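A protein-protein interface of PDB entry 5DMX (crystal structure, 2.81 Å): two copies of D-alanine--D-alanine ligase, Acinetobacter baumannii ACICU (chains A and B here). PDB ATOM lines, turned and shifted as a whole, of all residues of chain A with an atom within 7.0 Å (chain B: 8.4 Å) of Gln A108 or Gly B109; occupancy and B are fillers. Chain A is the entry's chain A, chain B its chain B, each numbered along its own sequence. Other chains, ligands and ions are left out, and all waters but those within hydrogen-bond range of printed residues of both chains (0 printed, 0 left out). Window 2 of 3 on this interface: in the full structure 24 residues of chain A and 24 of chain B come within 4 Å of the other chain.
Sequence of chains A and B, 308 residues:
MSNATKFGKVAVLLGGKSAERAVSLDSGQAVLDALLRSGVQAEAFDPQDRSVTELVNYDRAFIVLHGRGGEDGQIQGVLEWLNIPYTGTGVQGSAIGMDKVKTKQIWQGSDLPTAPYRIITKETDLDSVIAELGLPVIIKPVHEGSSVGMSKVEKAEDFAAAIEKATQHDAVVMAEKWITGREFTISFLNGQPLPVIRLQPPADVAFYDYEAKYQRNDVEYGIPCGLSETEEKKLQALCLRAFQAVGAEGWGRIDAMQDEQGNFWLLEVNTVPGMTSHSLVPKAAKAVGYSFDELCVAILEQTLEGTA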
ATOM      1  N   VAL A 101     -26.335   1.042  16.427  1.00  0.00           N
ATOM      2  CA  VAL A 101     -25.367  -0.031  16.738  1.00  0.00           C
ATOM      3  C   VAL A 101     -26.124  -1.322  17.031  1.00  0.00           C
ATOM      4  O   VAL A 101     -25.783  -2.380  16.474  1.00  0.00           O
ATOM      5  CB  VAL A 101     -24.306   0.312  17.845  1.00  0.00           C
ATOM      6  CG1 VAL A 101     -23.648   1.661  17.573  1.00  0.00           C
ATOM      7  CG2 VAL A 101     -24.860   0.267  19.264  1.00  0.00           C
ATOM      8  N   THR A 103     -29.256  -2.019  16.085  1.00  0.00           N
ATOM      9  CA  THR A 103     -29.950  -2.424  14.873  1.00  0.00           C
ATOM     10  C   THR A 103     -28.982  -3.139  13.942  1.00  0.00           C
ATOM     11  O   THR A 103     -29.354  -4.135  13.310  1.00  0.00           O
ATOM     12  CB  THR A 103     -30.585  -1.228  14.158  1.00  0.00           C
ATOM     13  OG1 THR A 103     -31.253  -0.416  15.122  1.00  0.00           O
ATOM     14  CG2 THR A 103     -31.610  -1.664  13.115  1.00  0.00           C
ATOM     15  N   LYS A 104     -27.746  -2.650  13.886  1.00  0.00           N
ATOM     16  CA  LYS A 104     -26.719  -3.276  13.058  1.00  0.00           C
ATOM     17  C   LYS A 104     -26.300  -4.611  13.599  1.00  0.00           C
ATOM     18  O   LYS A 104     -26.334  -5.598  12.870  1.00  0.00           O
ATOM     19  CB  LYS A 104     -25.495  -2.391  12.936  1.00  0.00           C
ATOM     20  CG  LYS A 104     -25.739  -1.162  12.074  1.00  0.00           C
ATOM     21  CD  LYS A 104     -24.543  -0.226  12.039  1.00  0.00           C
ATOM     22  CE  LYS A 104     -24.527   0.658  10.787  1.00  0.00           C
ATOM     23  NZ  LYS A 104     -23.715   0.084   9.679  1.00  0.00           N
ATOM     24  N   GLN A 105     -25.972  -4.651  14.885  1.00  0.00           N
ATOM     25  CA  GLN A 105     -25.698  -5.919  15.583  1.00  0.00           C
ATOM     26  C   GLN A 105     -26.732  -6.978  15.258  1.00  0.00           C
ATOM     27  O   GLN A 105     -26.356  -8.062  14.810  1.00  0.00           O
ATOM     28  CB  GLN A 105     -25.550  -5.740  17.105  1.00  0.00           C
ATOM     29  CG  GLN A 105     -24.210  -5.110  17.451  1.00  0.00           C
ATOM     30  CD  GLN A 105     -23.961  -4.814  18.939  1.00  0.00           C
ATOM     31  OE1 GLN A 105     -22.808  -4.858  19.403  1.00  0.00           O
ATOM     32  NE2 GLN A 105     -25.001  -4.479  19.684  1.00  0.00           N
ATOM     33  N   ILE A 106     -28.021  -6.673  15.373  1.00  0.00           N
ATOM     34  CA  ILE A 106     -29.005  -7.748  15.160  1.00  0.00           C
ATOM     35  C   ILE A 106     -29.185  -8.104  13.683  1.00  0.00           C
ATOM     36  O   ILE A 106     -29.621  -9.214  13.346  1.00  0.00           O
ATOM     37  CB  ILE A 106     -30.358  -7.598  15.933  1.00  0.00           C
ATOM     38  CG1 ILE A 106     -31.475  -7.035  15.096  1.00  0.00           C
ATOM     39  CG2 ILE A 106     -30.249  -6.817  17.231  1.00  0.00           C
ATOM     40  CD1 ILE A 106     -32.412  -8.115  14.646  1.00  0.00           C
ATOM     41  N   TRP A 107     -28.830  -7.162  12.815  1.00  0.00           N
ATOM     42  CA  TRP A 107     -28.811  -7.420  11.374  1.00  0.00           C
ATOM     43  C   TRP A 107     -27.625  -8.314  10.970  1.00  0.00           C
ATOM     44  O   TRP A 107     -27.842  -9.343  10.316  1.00  0.00           O
ATOM     45  CB  TRP A 107     -28.837  -6.103  10.576  1.00  0.00           C
ATOM     46  CG  TRP A 107     -30.215  -5.458  10.400  1.00  0.00           C
ATOM     47  CD1 TRP A 107     -31.444  -6.074  10.440  1.00  0.00           C
ATOM     48  CD2 TRP A 107     -30.468  -4.084  10.095  1.00  0.00           C
ATOM     49  NE1 TRP A 107     -32.437  -5.152  10.217  1.00  0.00           N
ATOM     50  CE2 TRP A 107     -31.866  -3.929   9.995  1.00  0.00           C
ATOM     51  CE3 TRP A 107     -29.644  -2.969   9.920  1.00  0.00           C
ATOM     52  CZ2 TRP A 107     -32.457  -2.717   9.721  1.00  0.00           C
ATOM     53  CZ3 TRP A 107     -30.225  -1.762   9.660  1.00  0.00           C
ATOM     54  CH2 TRP A 107     -31.626  -1.640   9.564  1.00  0.00           C
ATOM     55  N   GLN A 108     -26.400  -7.943  11.367  1.00  0.00           N
ATOM     56  CA  GLN A 108     -25.207  -8.821  11.211  1.00  0.00           C
ATOM     57  C   GLN A 108     -25.550 -10.229  11.717  1.00  0.00           C
ATOM     58  O   GLN A 108     -25.481 -11.209  10.943  1.00  0.00           O
ATOM     59  CB  GLN A 108     -23.980  -8.320  11.970  1.00  0.00           C
ATOM     60  CG  GLN A 108     -23.563  -6.886  11.672  1.00  0.00           C
ATOM     61  CD  GLN A 108     -22.377  -6.424  12.505  1.00  0.00           C
ATOM     62  OE1 GLN A 108     -22.330  -6.653  13.720  1.00  0.00           O
ATOM     63  NE2 GLN A 108     -21.437  -5.749  11.876  1.00  0.00           N
ATOM     64  N   GLY A 109     -26.052 -10.305  12.954  1.00  0.00           N
ATOM     65  CA  GLY A 109     -26.558 -11.557  13.515  1.00  0.00           C
ATOM     66  C   GLY A 109     -27.679 -12.304  12.782  1.00  0.00           C
ATOM     67  O   GLY A 109     -28.024 -13.421  13.183  1.00  0.00           O
ATOM     68  N   SER A 110     -28.273 -11.719  11.735  1.00  0.00           N
ATOM     69  CA  SER A 110     -29.282 -12.410  10.917  1.00  0.00           C
ATOM     70  C   SER A 110     -28.815 -12.618   9.474  1.00  0.00           C
ATOM     71  O   SER A 110     -29.647 -12.861   8.574  1.00  0.00           O
ATOM     72  CB  SER A 110     -30.609 -11.627  10.933  1.00  0.00           C
ATOM     73  OG  SER A 110     -31.052 -11.355  12.253  1.00  0.00           O
ATOM     74  N   ASP A 111     -27.502 -12.513   9.249  1.00  0.00           N
ATOM     75  CA  ASP A 111     -26.909 -12.682   7.921  1.00  0.00           C
ATOM     76  C   ASP A 111     -27.416 -11.611   6.915  1.00  0.00           C
ATOM     77  O   ASP A 111     -27.764 -11.938   5.771  1.00  0.00           O
ATOM     78  CB  ASP A 111     -27.170 -14.122   7.410  1.00  0.00           C
ATOM     79  CG  ASP A 111     -26.158 -14.586   6.370  1.00  0.00           C
ATOM     80  OD1 ASP A 111     -25.015 -14.073   6.332  1.00  0.00           O
ATOM     81  OD2 ASP A 111     -26.511 -15.490   5.584  1.00  0.00           O
ATOM     82  N   LEU A 112     -27.485 -10.351   7.364  1.00  0.00           N
ATOM     83  CA  LEU A 112     -28.026  -9.242   6.573  1.00  0.00           C
ATOM     84  C   LEU A 112     -26.991  -8.133   6.401  1.00  0.00           C
ATOM     85  O   LEU A 112     -26.221  -7.839   7.324  1.00  0.00           O
ATOM     86  CB  LEU A 112     -29.309  -8.682   7.216  1.00  0.00           C
ATOM     87  CG  LEU A 112     -30.701  -9.097   6.706  1.00  0.00           C
ATOM     88  CD1 LEU A 112     -30.800 -10.471   6.066  1.00  0.00           C
ATOM     89  CD2 LEU A 112     -31.723  -9.002   7.825  1.00  0.00           C
ATOM     90  N   PRO A 113     -26.979  -7.500   5.210  1.00  0.00           N
ATOM     91  CA  PRO A 113     -25.884  -6.620   4.824  1.00  0.00           C
ATOM     92  C   PRO A 113     -25.994  -5.251   5.438  1.00  0.00           C
ATOM     93  O   PRO A 113     -27.054  -4.658   5.413  1.00  0.00           O
ATOM     94  CB  PRO A 113     -26.037  -6.525   3.316  1.00  0.00           C
ATOM     95  CG  PRO A 113     -27.492  -6.692   3.086  1.00  0.00           C
ATOM     96  CD  PRO A 113     -28.011  -7.587   4.161  1.00  0.00           C
ATOM     97  N   THR A 114     -24.885  -4.744   5.965  1.00  0.00           N
ATOM     98  CA  THR A 114     -24.852  -3.406   6.544  1.00  0.00           C
ATOM     99  C   THR A 114     -23.405  -2.971   6.713  1.00  0.00           C
ATOM    100  O   THR A 114     -22.511  -3.789   6.960  1.00  0.00           O
ATOM    101  CB  THR A 114     -25.624  -3.341   7.893  1.00  0.00           C
ATOM    102  OG1 THR A 114     -25.248  -2.169   8.633  1.00  0.00           O
ATOM    103  CG2 THR A 114     -25.346  -4.577   8.757  1.00  0.00           C
ATOM    104  N   ALA A 115     -23.172  -1.673   6.586  1.00  0.00           N
ATOM    105  CA  ALA A 115     -21.805  -1.159   6.638  1.00  0.00           C
ATOM    106  C   ALA A 115     -21.129  -1.612   7.915  1.00  0.00           C
ATOM    107  O   ALA A 115     -21.767  -1.612   8.969  1.00  0.00           O
ATOM    108  CB  ALA A 115     -21.805   0.346   6.576  1.00  0.00           C
ATOM    109  N   PRO A 116     -19.868  -2.069   7.817  1.00  0.00           N
ATOM    110  CA  PRO A 116     -18.992  -2.123   8.987  1.00  0.00           C
ATOM    111  C   PRO A 116     -18.902  -0.811   9.762  1.00  0.00           C
ATOM    112  O   PRO A 116     -19.219   0.256   9.235  1.00  0.00           O
ATOM    113  CB  PRO A 116     -17.656  -2.477   8.375  1.00  0.00           C
ATOM    114  CG  PRO A 116     -18.015  -3.382   7.241  1.00  0.00           C
ATOM    115  CD  PRO A 116     -19.375  -2.963   6.749  1.00  0.00           C
ATOM    116  N   TYR A 117     -18.545  -0.924  11.032  1.00  0.00           N
ATOM    117  CA  TYR A 117     -18.623   0.197  11.971  1.00  0.00           C
ATOM    118  C   TYR A 117     -17.752  -0.112  13.164  1.00  0.00           C
ATOM    119  O   TYR A 117     -17.455  -1.267  13.410  1.00  0.00           O
ATOM    120  CB  TYR A 117     -20.087   0.449  12.434  1.00  0.00           C
ATOM    121  CG  TYR A 117     -20.614  -0.585  13.406  1.00  0.00           C
ATOM    122  CD1 TYR A 117     -21.093  -1.805  12.936  1.00  0.00           C
ATOM    123  CD2 TYR A 117     -20.611  -0.357  14.794  1.00  0.00           C
ATOM    124  CE1 TYR A 117     -21.544  -2.768  13.808  1.00  0.00           C
ATOM    125  CE2 TYR A 117     -21.063  -1.318  15.674  1.00  0.00           C
ATOM    126  CZ  TYR A 117     -21.526  -2.515  15.167  1.00  0.00           C
ATOM    127  OH  TYR A 117     -21.973  -3.485  16.000  1.00  0.00           O
ATOM    128  N   LYS B 102     -33.082 -12.886  20.401  1.00  0.00           N
ATOM    129  CA  LYS B 102     -32.533 -11.537  20.302  1.00  0.00           C
ATOM    130  C   LYS B 102     -31.224 -11.400  21.053  1.00  0.00           C
ATOM    131  O   LYS B 102     -30.324 -10.705  20.601  1.00  0.00           O
ATOM    132  CB  LYS B 102     -33.528 -10.508  20.807  1.00  0.00           C
ATOM    133  CG  LYS B 102     -34.763 -10.360  19.932  1.00  0.00           C
ATOM    134  CD  LYS B 102     -34.621  -9.244  18.895  1.00  0.00           C
ATOM    135  CE  LYS B 102     -35.429  -9.513  17.632  1.00  0.00           C
ATOM    136  NZ  LYS B 102     -36.784 -10.091  17.851  1.00  0.00           N
ATOM    137  N   THR B 103     -31.115 -12.057  22.201  1.00  0.00           N
ATOM    138  CA  THR B 103     -29.880 -12.018  22.972  1.00  0.00           C
ATOM    139  C   THR B 103     -28.767 -12.706  22.195  1.00  0.00           C
ATOM    140  O   THR B 103     -27.617 -12.237  22.190  1.00  0.00           O
ATOM    141  CB  THR B 103     -30.051 -12.670  24.347  1.00  0.00           C
ATOM    142  OG1 THR B 103     -31.260 -12.199  24.938  1.00  0.00           O
ATOM    143  CG2 THR B 103     -28.907 -12.327  25.277  1.00  0.00           C
ATOM    144  N   LYS B 104     -29.124 -13.796  21.516  1.00  0.00           N
ATOM    145  CA  LYS B 104     -28.159 -14.527  20.702  1.00  0.00           C
ATOM    146  C   LYS B 104     -27.753 -13.741  19.481  1.00  0.00           C
ATOM    147  O   LYS B 104     -26.559 -13.560  19.241  1.00  0.00           O
ATOM    148  CB  LYS B 104     -28.709 -15.871  20.271  1.00  0.00           C
ATOM    149  CG  LYS B 104     -28.799 -16.846  21.428  1.00  0.00           C
ATOM    150  CD  LYS B 104     -29.453 -18.150  21.027  1.00  0.00           C
ATOM    151  CE  LYS B 104     -29.048 -19.299  21.956  1.00  0.00           C
ATOM    152  NZ  LYS B 104     -27.884 -20.082  21.464  1.00  0.00           N
ATOM    153  N   GLN B 105     -28.743 -13.234  18.750  1.00  0.00           N
ATOM    154  CA  GLN B 105     -28.482 -12.347  17.605  1.00  0.00           C
ATOM    155  C   GLN B 105     -27.476 -11.284  17.962  1.00  0.00           C
ATOM    156  O   GLN B 105     -26.491 -11.148  17.256  1.00  0.00           O
ATOM    157  CB  GLN B 105     -29.777 -11.742  17.038  1.00  0.00           C
ATOM    158  CG  GLN B 105     -30.535 -12.781  16.215  1.00  0.00           C
ATOM    159  CD  GLN B 105     -31.931 -12.417  15.733  1.00  0.00           C
ATOM    160  OE1 GLN B 105     -32.427 -13.060  14.805  1.00  0.00           O
ATOM    161  NE2 GLN B 105     -32.589 -11.436  16.349  1.00  0.00           N
ATOM    162  N   ILE B 106     -27.672 -10.568  19.069  1.00  0.00           N
ATOM    163  CA  ILE B 106     -26.783  -9.426  19.322  1.00  0.00           C
ATOM    164  C   ILE B 106     -25.431  -9.876  19.827  1.00  0.00           C
ATOM    165  O   ILE B 106     -24.443  -9.157  19.673  1.00  0.00           O
ATOM    166  CB  ILE B 106     -27.410  -8.132  20.011  1.00  0.00           C
ATOM    167  CG1 ILE B 106     -26.933  -7.802  21.402  1.00  0.00           C
ATOM    168  CG2 ILE B 106     -28.908  -8.093  20.071  1.00  0.00           C
ATOM    169  CD1 ILE B 106     -26.731  -6.310  21.619  1.00  0.00           C
ATOM    170  N   TRP B 107     -25.381 -11.097  20.359  1.00  0.00           N
ATOM    171  CA  TRP B 107     -24.104 -11.730  20.729  1.00  0.00           C
ATOM    172  C   TRP B 107     -23.308 -12.201  19.496  1.00  0.00           C
ATOM    173  O   TRP B 107     -22.135 -11.812  19.343  1.00  0.00           O
ATOM    174  CB  TRP B 107     -24.311 -12.868  21.725  1.00  0.00           C
ATOM    175  CG  TRP B 107     -24.498 -12.444  23.170  1.00  0.00           C
ATOM    176  CD1 TRP B 107     -24.052 -11.301  23.772  1.00  0.00           C
ATOM    177  CD2 TRP B 107     -25.119 -13.224  24.203  1.00  0.00           C
ATOM    178  NE1 TRP B 107     -24.383 -11.315  25.104  1.00  0.00           N
ATOM    179  CE2 TRP B 107     -25.020 -12.491  25.395  1.00  0.00           C
ATOM    180  CE3 TRP B 107     -25.744 -14.481  24.231  1.00  0.00           C
ATOM    181  CZ2 TRP B 107     -25.531 -12.962  26.600  1.00  0.00           C
ATOM    182  CZ3 TRP B 107     -26.263 -14.948  25.433  1.00  0.00           C
ATOM    183  CH2 TRP B 107     -26.154 -14.192  26.596  1.00  0.00           C
ATOM    184  N   GLN B 108     -23.938 -12.975  18.601  1.00  0.00           N
ATOM    185  CA  GLN B 108     -23.332 -13.313  17.280  1.00  0.00           C
ATOM    186  C   GLN B 108     -22.793 -12.025  16.635  1.00  0.00           C
ATOM    187  O   GLN B 108     -21.608 -11.926  16.316  1.00  0.00           O
ATOM    188  CB  GLN B 108     -24.325 -13.995  16.327  1.00  0.00           C
ATOM    189  CG  GLN B 108     -25.023 -15.234  16.876  1.00  0.00           C
ATOM    190  CD  GLN B 108     -26.041 -15.823  15.921  1.00  0.00           C
ATOM    191  OE1 GLN B 108     -26.834 -15.091  15.317  1.00  0.00           O
ATOM    192  NE2 GLN B 108     -26.050 -17.139  15.797  1.00  0.00           N
ATOM    193  N   GLY B 109     -23.655 -11.016  16.534  1.00  0.00           N
ATOM    194  CA  GLY B 109     -23.278  -9.693  16.039  1.00  0.00           C
ATOM    195  C   GLY B 109     -22.168  -8.936  16.765  1.00  0.00           C
ATOM    196  O   GLY B 109     -21.746  -7.879  16.283  1.00  0.00           O
ATOM    197  N   SER B 110     -21.694  -9.441  17.909  1.00  0.00           N
ATOM    198  CA  SER B 110     -20.551  -8.843  18.618  1.00  0.00           C
ATOM    199  C   SER B 110     -19.348  -9.802  18.676  1.00  0.00           C
ATOM    200  O   SER B 110     -18.446  -9.589  19.482  1.00  0.00           O
ATOM    201  CB  SER B 110     -20.969  -8.428  20.035  1.00  0.00           C
ATOM    202  OG  SER B 110     -22.139  -7.613  20.030  1.00  0.00           O
ATOM    203  N   ASP B 111     -19.341 -10.821  17.806  1.00  0.00           N
ATOM    204  CA  ASP B 111     -18.300 -11.869  17.750  1.00  0.00           C
ATOM    205  C   ASP B 111     -18.109 -12.569  19.092  1.00  0.00           C
ATOM    206  O   ASP B 111     -16.987 -12.754  19.579  1.00  0.00           O
ATOM    207  CB  ASP B 111     -16.950 -11.372  17.155  1.00  0.00           C
ATOM    208  CG  ASP B 111     -16.091 -12.510  16.571  1.00  0.00           C
ATOM    209  OD1 ASP B 111     -16.635 -13.572  16.173  1.00  0.00           O
ATOM    210  OD2 ASP B 111     -14.853 -12.326  16.504  1.00  0.00           O
ATOM    211  N   LEU B 112     -19.237 -12.994  19.639  1.00  0.00           N
ATOM    212  CA  LEU B 112     -19.283 -13.691  20.897  1.00  0.00           C
ATOM    213  C   LEU B 112     -19.903 -15.088  20.728  1.00  0.00           C
ATOM    214  O   LEU B 112     -20.887 -15.266  19.986  1.00  0.00           O
ATOM    215  CB  LEU B 112     -20.057 -12.863  21.941  1.00  0.00           C
ATOM    216  CG  LEU B 112     -19.310 -11.994  22.975  1.00  0.00           C
ATOM    217  CD1 LEU B 112     -17.941 -11.480  22.550  1.00  0.00           C
ATOM    218  CD2 LEU B 112     -20.170 -10.815  23.407  1.00  0.00           C
ATOM    219  N   PRO B 113     -19.339 -16.085  21.449  1.00  0.00           N
ATOM    220  CA  PRO B 113     -19.724 -17.475  21.267  1.00  0.00           C
ATOM    221  C   PRO B 113     -21.062 -17.865  21.860  1.00  0.00           C
ATOM    222  O   PRO B 113     -21.347 -17.540  22.994  1.00  0.00           O
ATOM    223  CB  PRO B 113     -18.614 -18.212  21.981  1.00  0.00           C
ATOM    224  CG  PRO B 113     -18.227 -17.306  23.085  1.00  0.00           C
ATOM    225  CD  PRO B 113     -18.448 -15.915  22.615  1.00  0.00           C
ATOM    226  N   THR B 114     -21.864 -18.578  21.095  1.00  0.00           N
ATOM    227  CA  THR B 114     -23.158 -19.052  21.576  1.00  0.00           C
ATOM    228  C   THR B 114     -23.670 -20.162  20.652  1.00  0.00           C
ATOM    229  O   THR B 114     -23.441 -20.151  19.445  1.00  0.00           O
ATOM    230  CB  THR B 114     -24.194 -17.886  21.709  1.00  0.00           C
ATOM    231  OG1 THR B 114     -25.541 -18.398  21.785  1.00  0.00           O
ATOM    232  CG2 THR B 114     -24.098 -16.929  20.533  1.00  0.00           C
ATOM    233  N   ALA B 245     -22.447  -5.826  25.722  1.00  0.00           N
ATOM    234  CA  ALA B 245     -22.982  -6.008  24.375  1.00  0.00           C
ATOM    235  C   ALA B 245     -24.494  -5.817  24.307  1.00  0.00           C
ATOM    236  O   ALA B 245     -24.961  -5.093  23.452  1.00  0.00           O
ATOM    237  CB  ALA B 245     -22.625  -7.387  23.846  1.00  0.00           C
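OE1 of Gln A105 lies within hydrogen-bond range of OG of Ser B110 (2.9 Å). The side-chain hydroxyl (OG) of Ser A110 sits at hydrogen-bond distance from the side-chain amide oxygen (OE1) of Gln B105, at 3.4 Å. O of Gly B109 sits close to OE1 of Gln A108, at 2.9 Å. O of Gly A109 lies close to OE1 of Gln B108.
O of Ile A106 sits at hydrogen-bond distance from OG of Ser A110 (2.8 Å). The side-chain hydroxyl (OG) of Ser B110 sits at hydrogen-bond distance from the backbone carbonyl oxygen (O) of Ile B106, 2.8 Å away.
O of Gln A105 touches O of Gln B105, at 3.9 Å. Ile B106 touches Gln A105. CA of Gly B109 touches O of Gln A105 (3.7 Å). O of Ala B245 touches NE2 of Gln A105 (3.8 Å). CD1 of Ile A106 touches NE2 of Gln B105, 3.7 Å away. Ile A106 touches Ile B106. Gln B105 touches Gly A109.
Of the printed residues of chain A, Gln B105 touches Gln A105 (3.9 Å), Ile A106 (3.7 Å), Gly A109 (3.8 Å) and Ser A110 (3.4 Å). Of the printed residues of chain A, Ile B106 touches Gln A105 and Ile A106. Of the printed residues of chain A, Gly B109 touches Gln A105 and Gln A108. Of the printed residues of chain A, Ser B110 touches Gln A105 (2.9 Å). The nearest residue of chain B that does not touch Gln A108 is Ser B110 (5.1 Å). The nearest residue of chain A that does not touch Gly B109 is Gly A109 (4.2 Å). The nearest printed residue of chain A that does not touch Ser B110 is Gln A108 (5.1 Å).
Of the 14 printed residues of chain B, 6 touch a printed residue of chain A. Printed residues of chain B that touch a printed residue of chain A: Gln B105, Ile B106, Gln B108, Gly B109, Ser B110 and Ala B245. Along chain B the printed residues that touch a printed residue of chain A span positions 105 to 245. Among the printed residues, 11 pairs touch across the chains. Among the printed residues, no Asp or Glu carboxylate lies within 4 Å of a Lys or Arg side-chain nitrogen of the other chain.
Gln A105 touches Ile B106, and with the chains exchanged Ile A106 touches Gln B105. Gln A105 touches Gly B109, and with the chains exchanged Gly A109 touches Gln B105. Ile B106 touches its own counterpart, Ile A106. Gln A108 touches Gly B109, and with the chains exchanged Gly A109 touches Gln B108. Of the 11 pairs that touch across the chains among the printed residues, 10 have their exchanged pair printed and touching as well.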
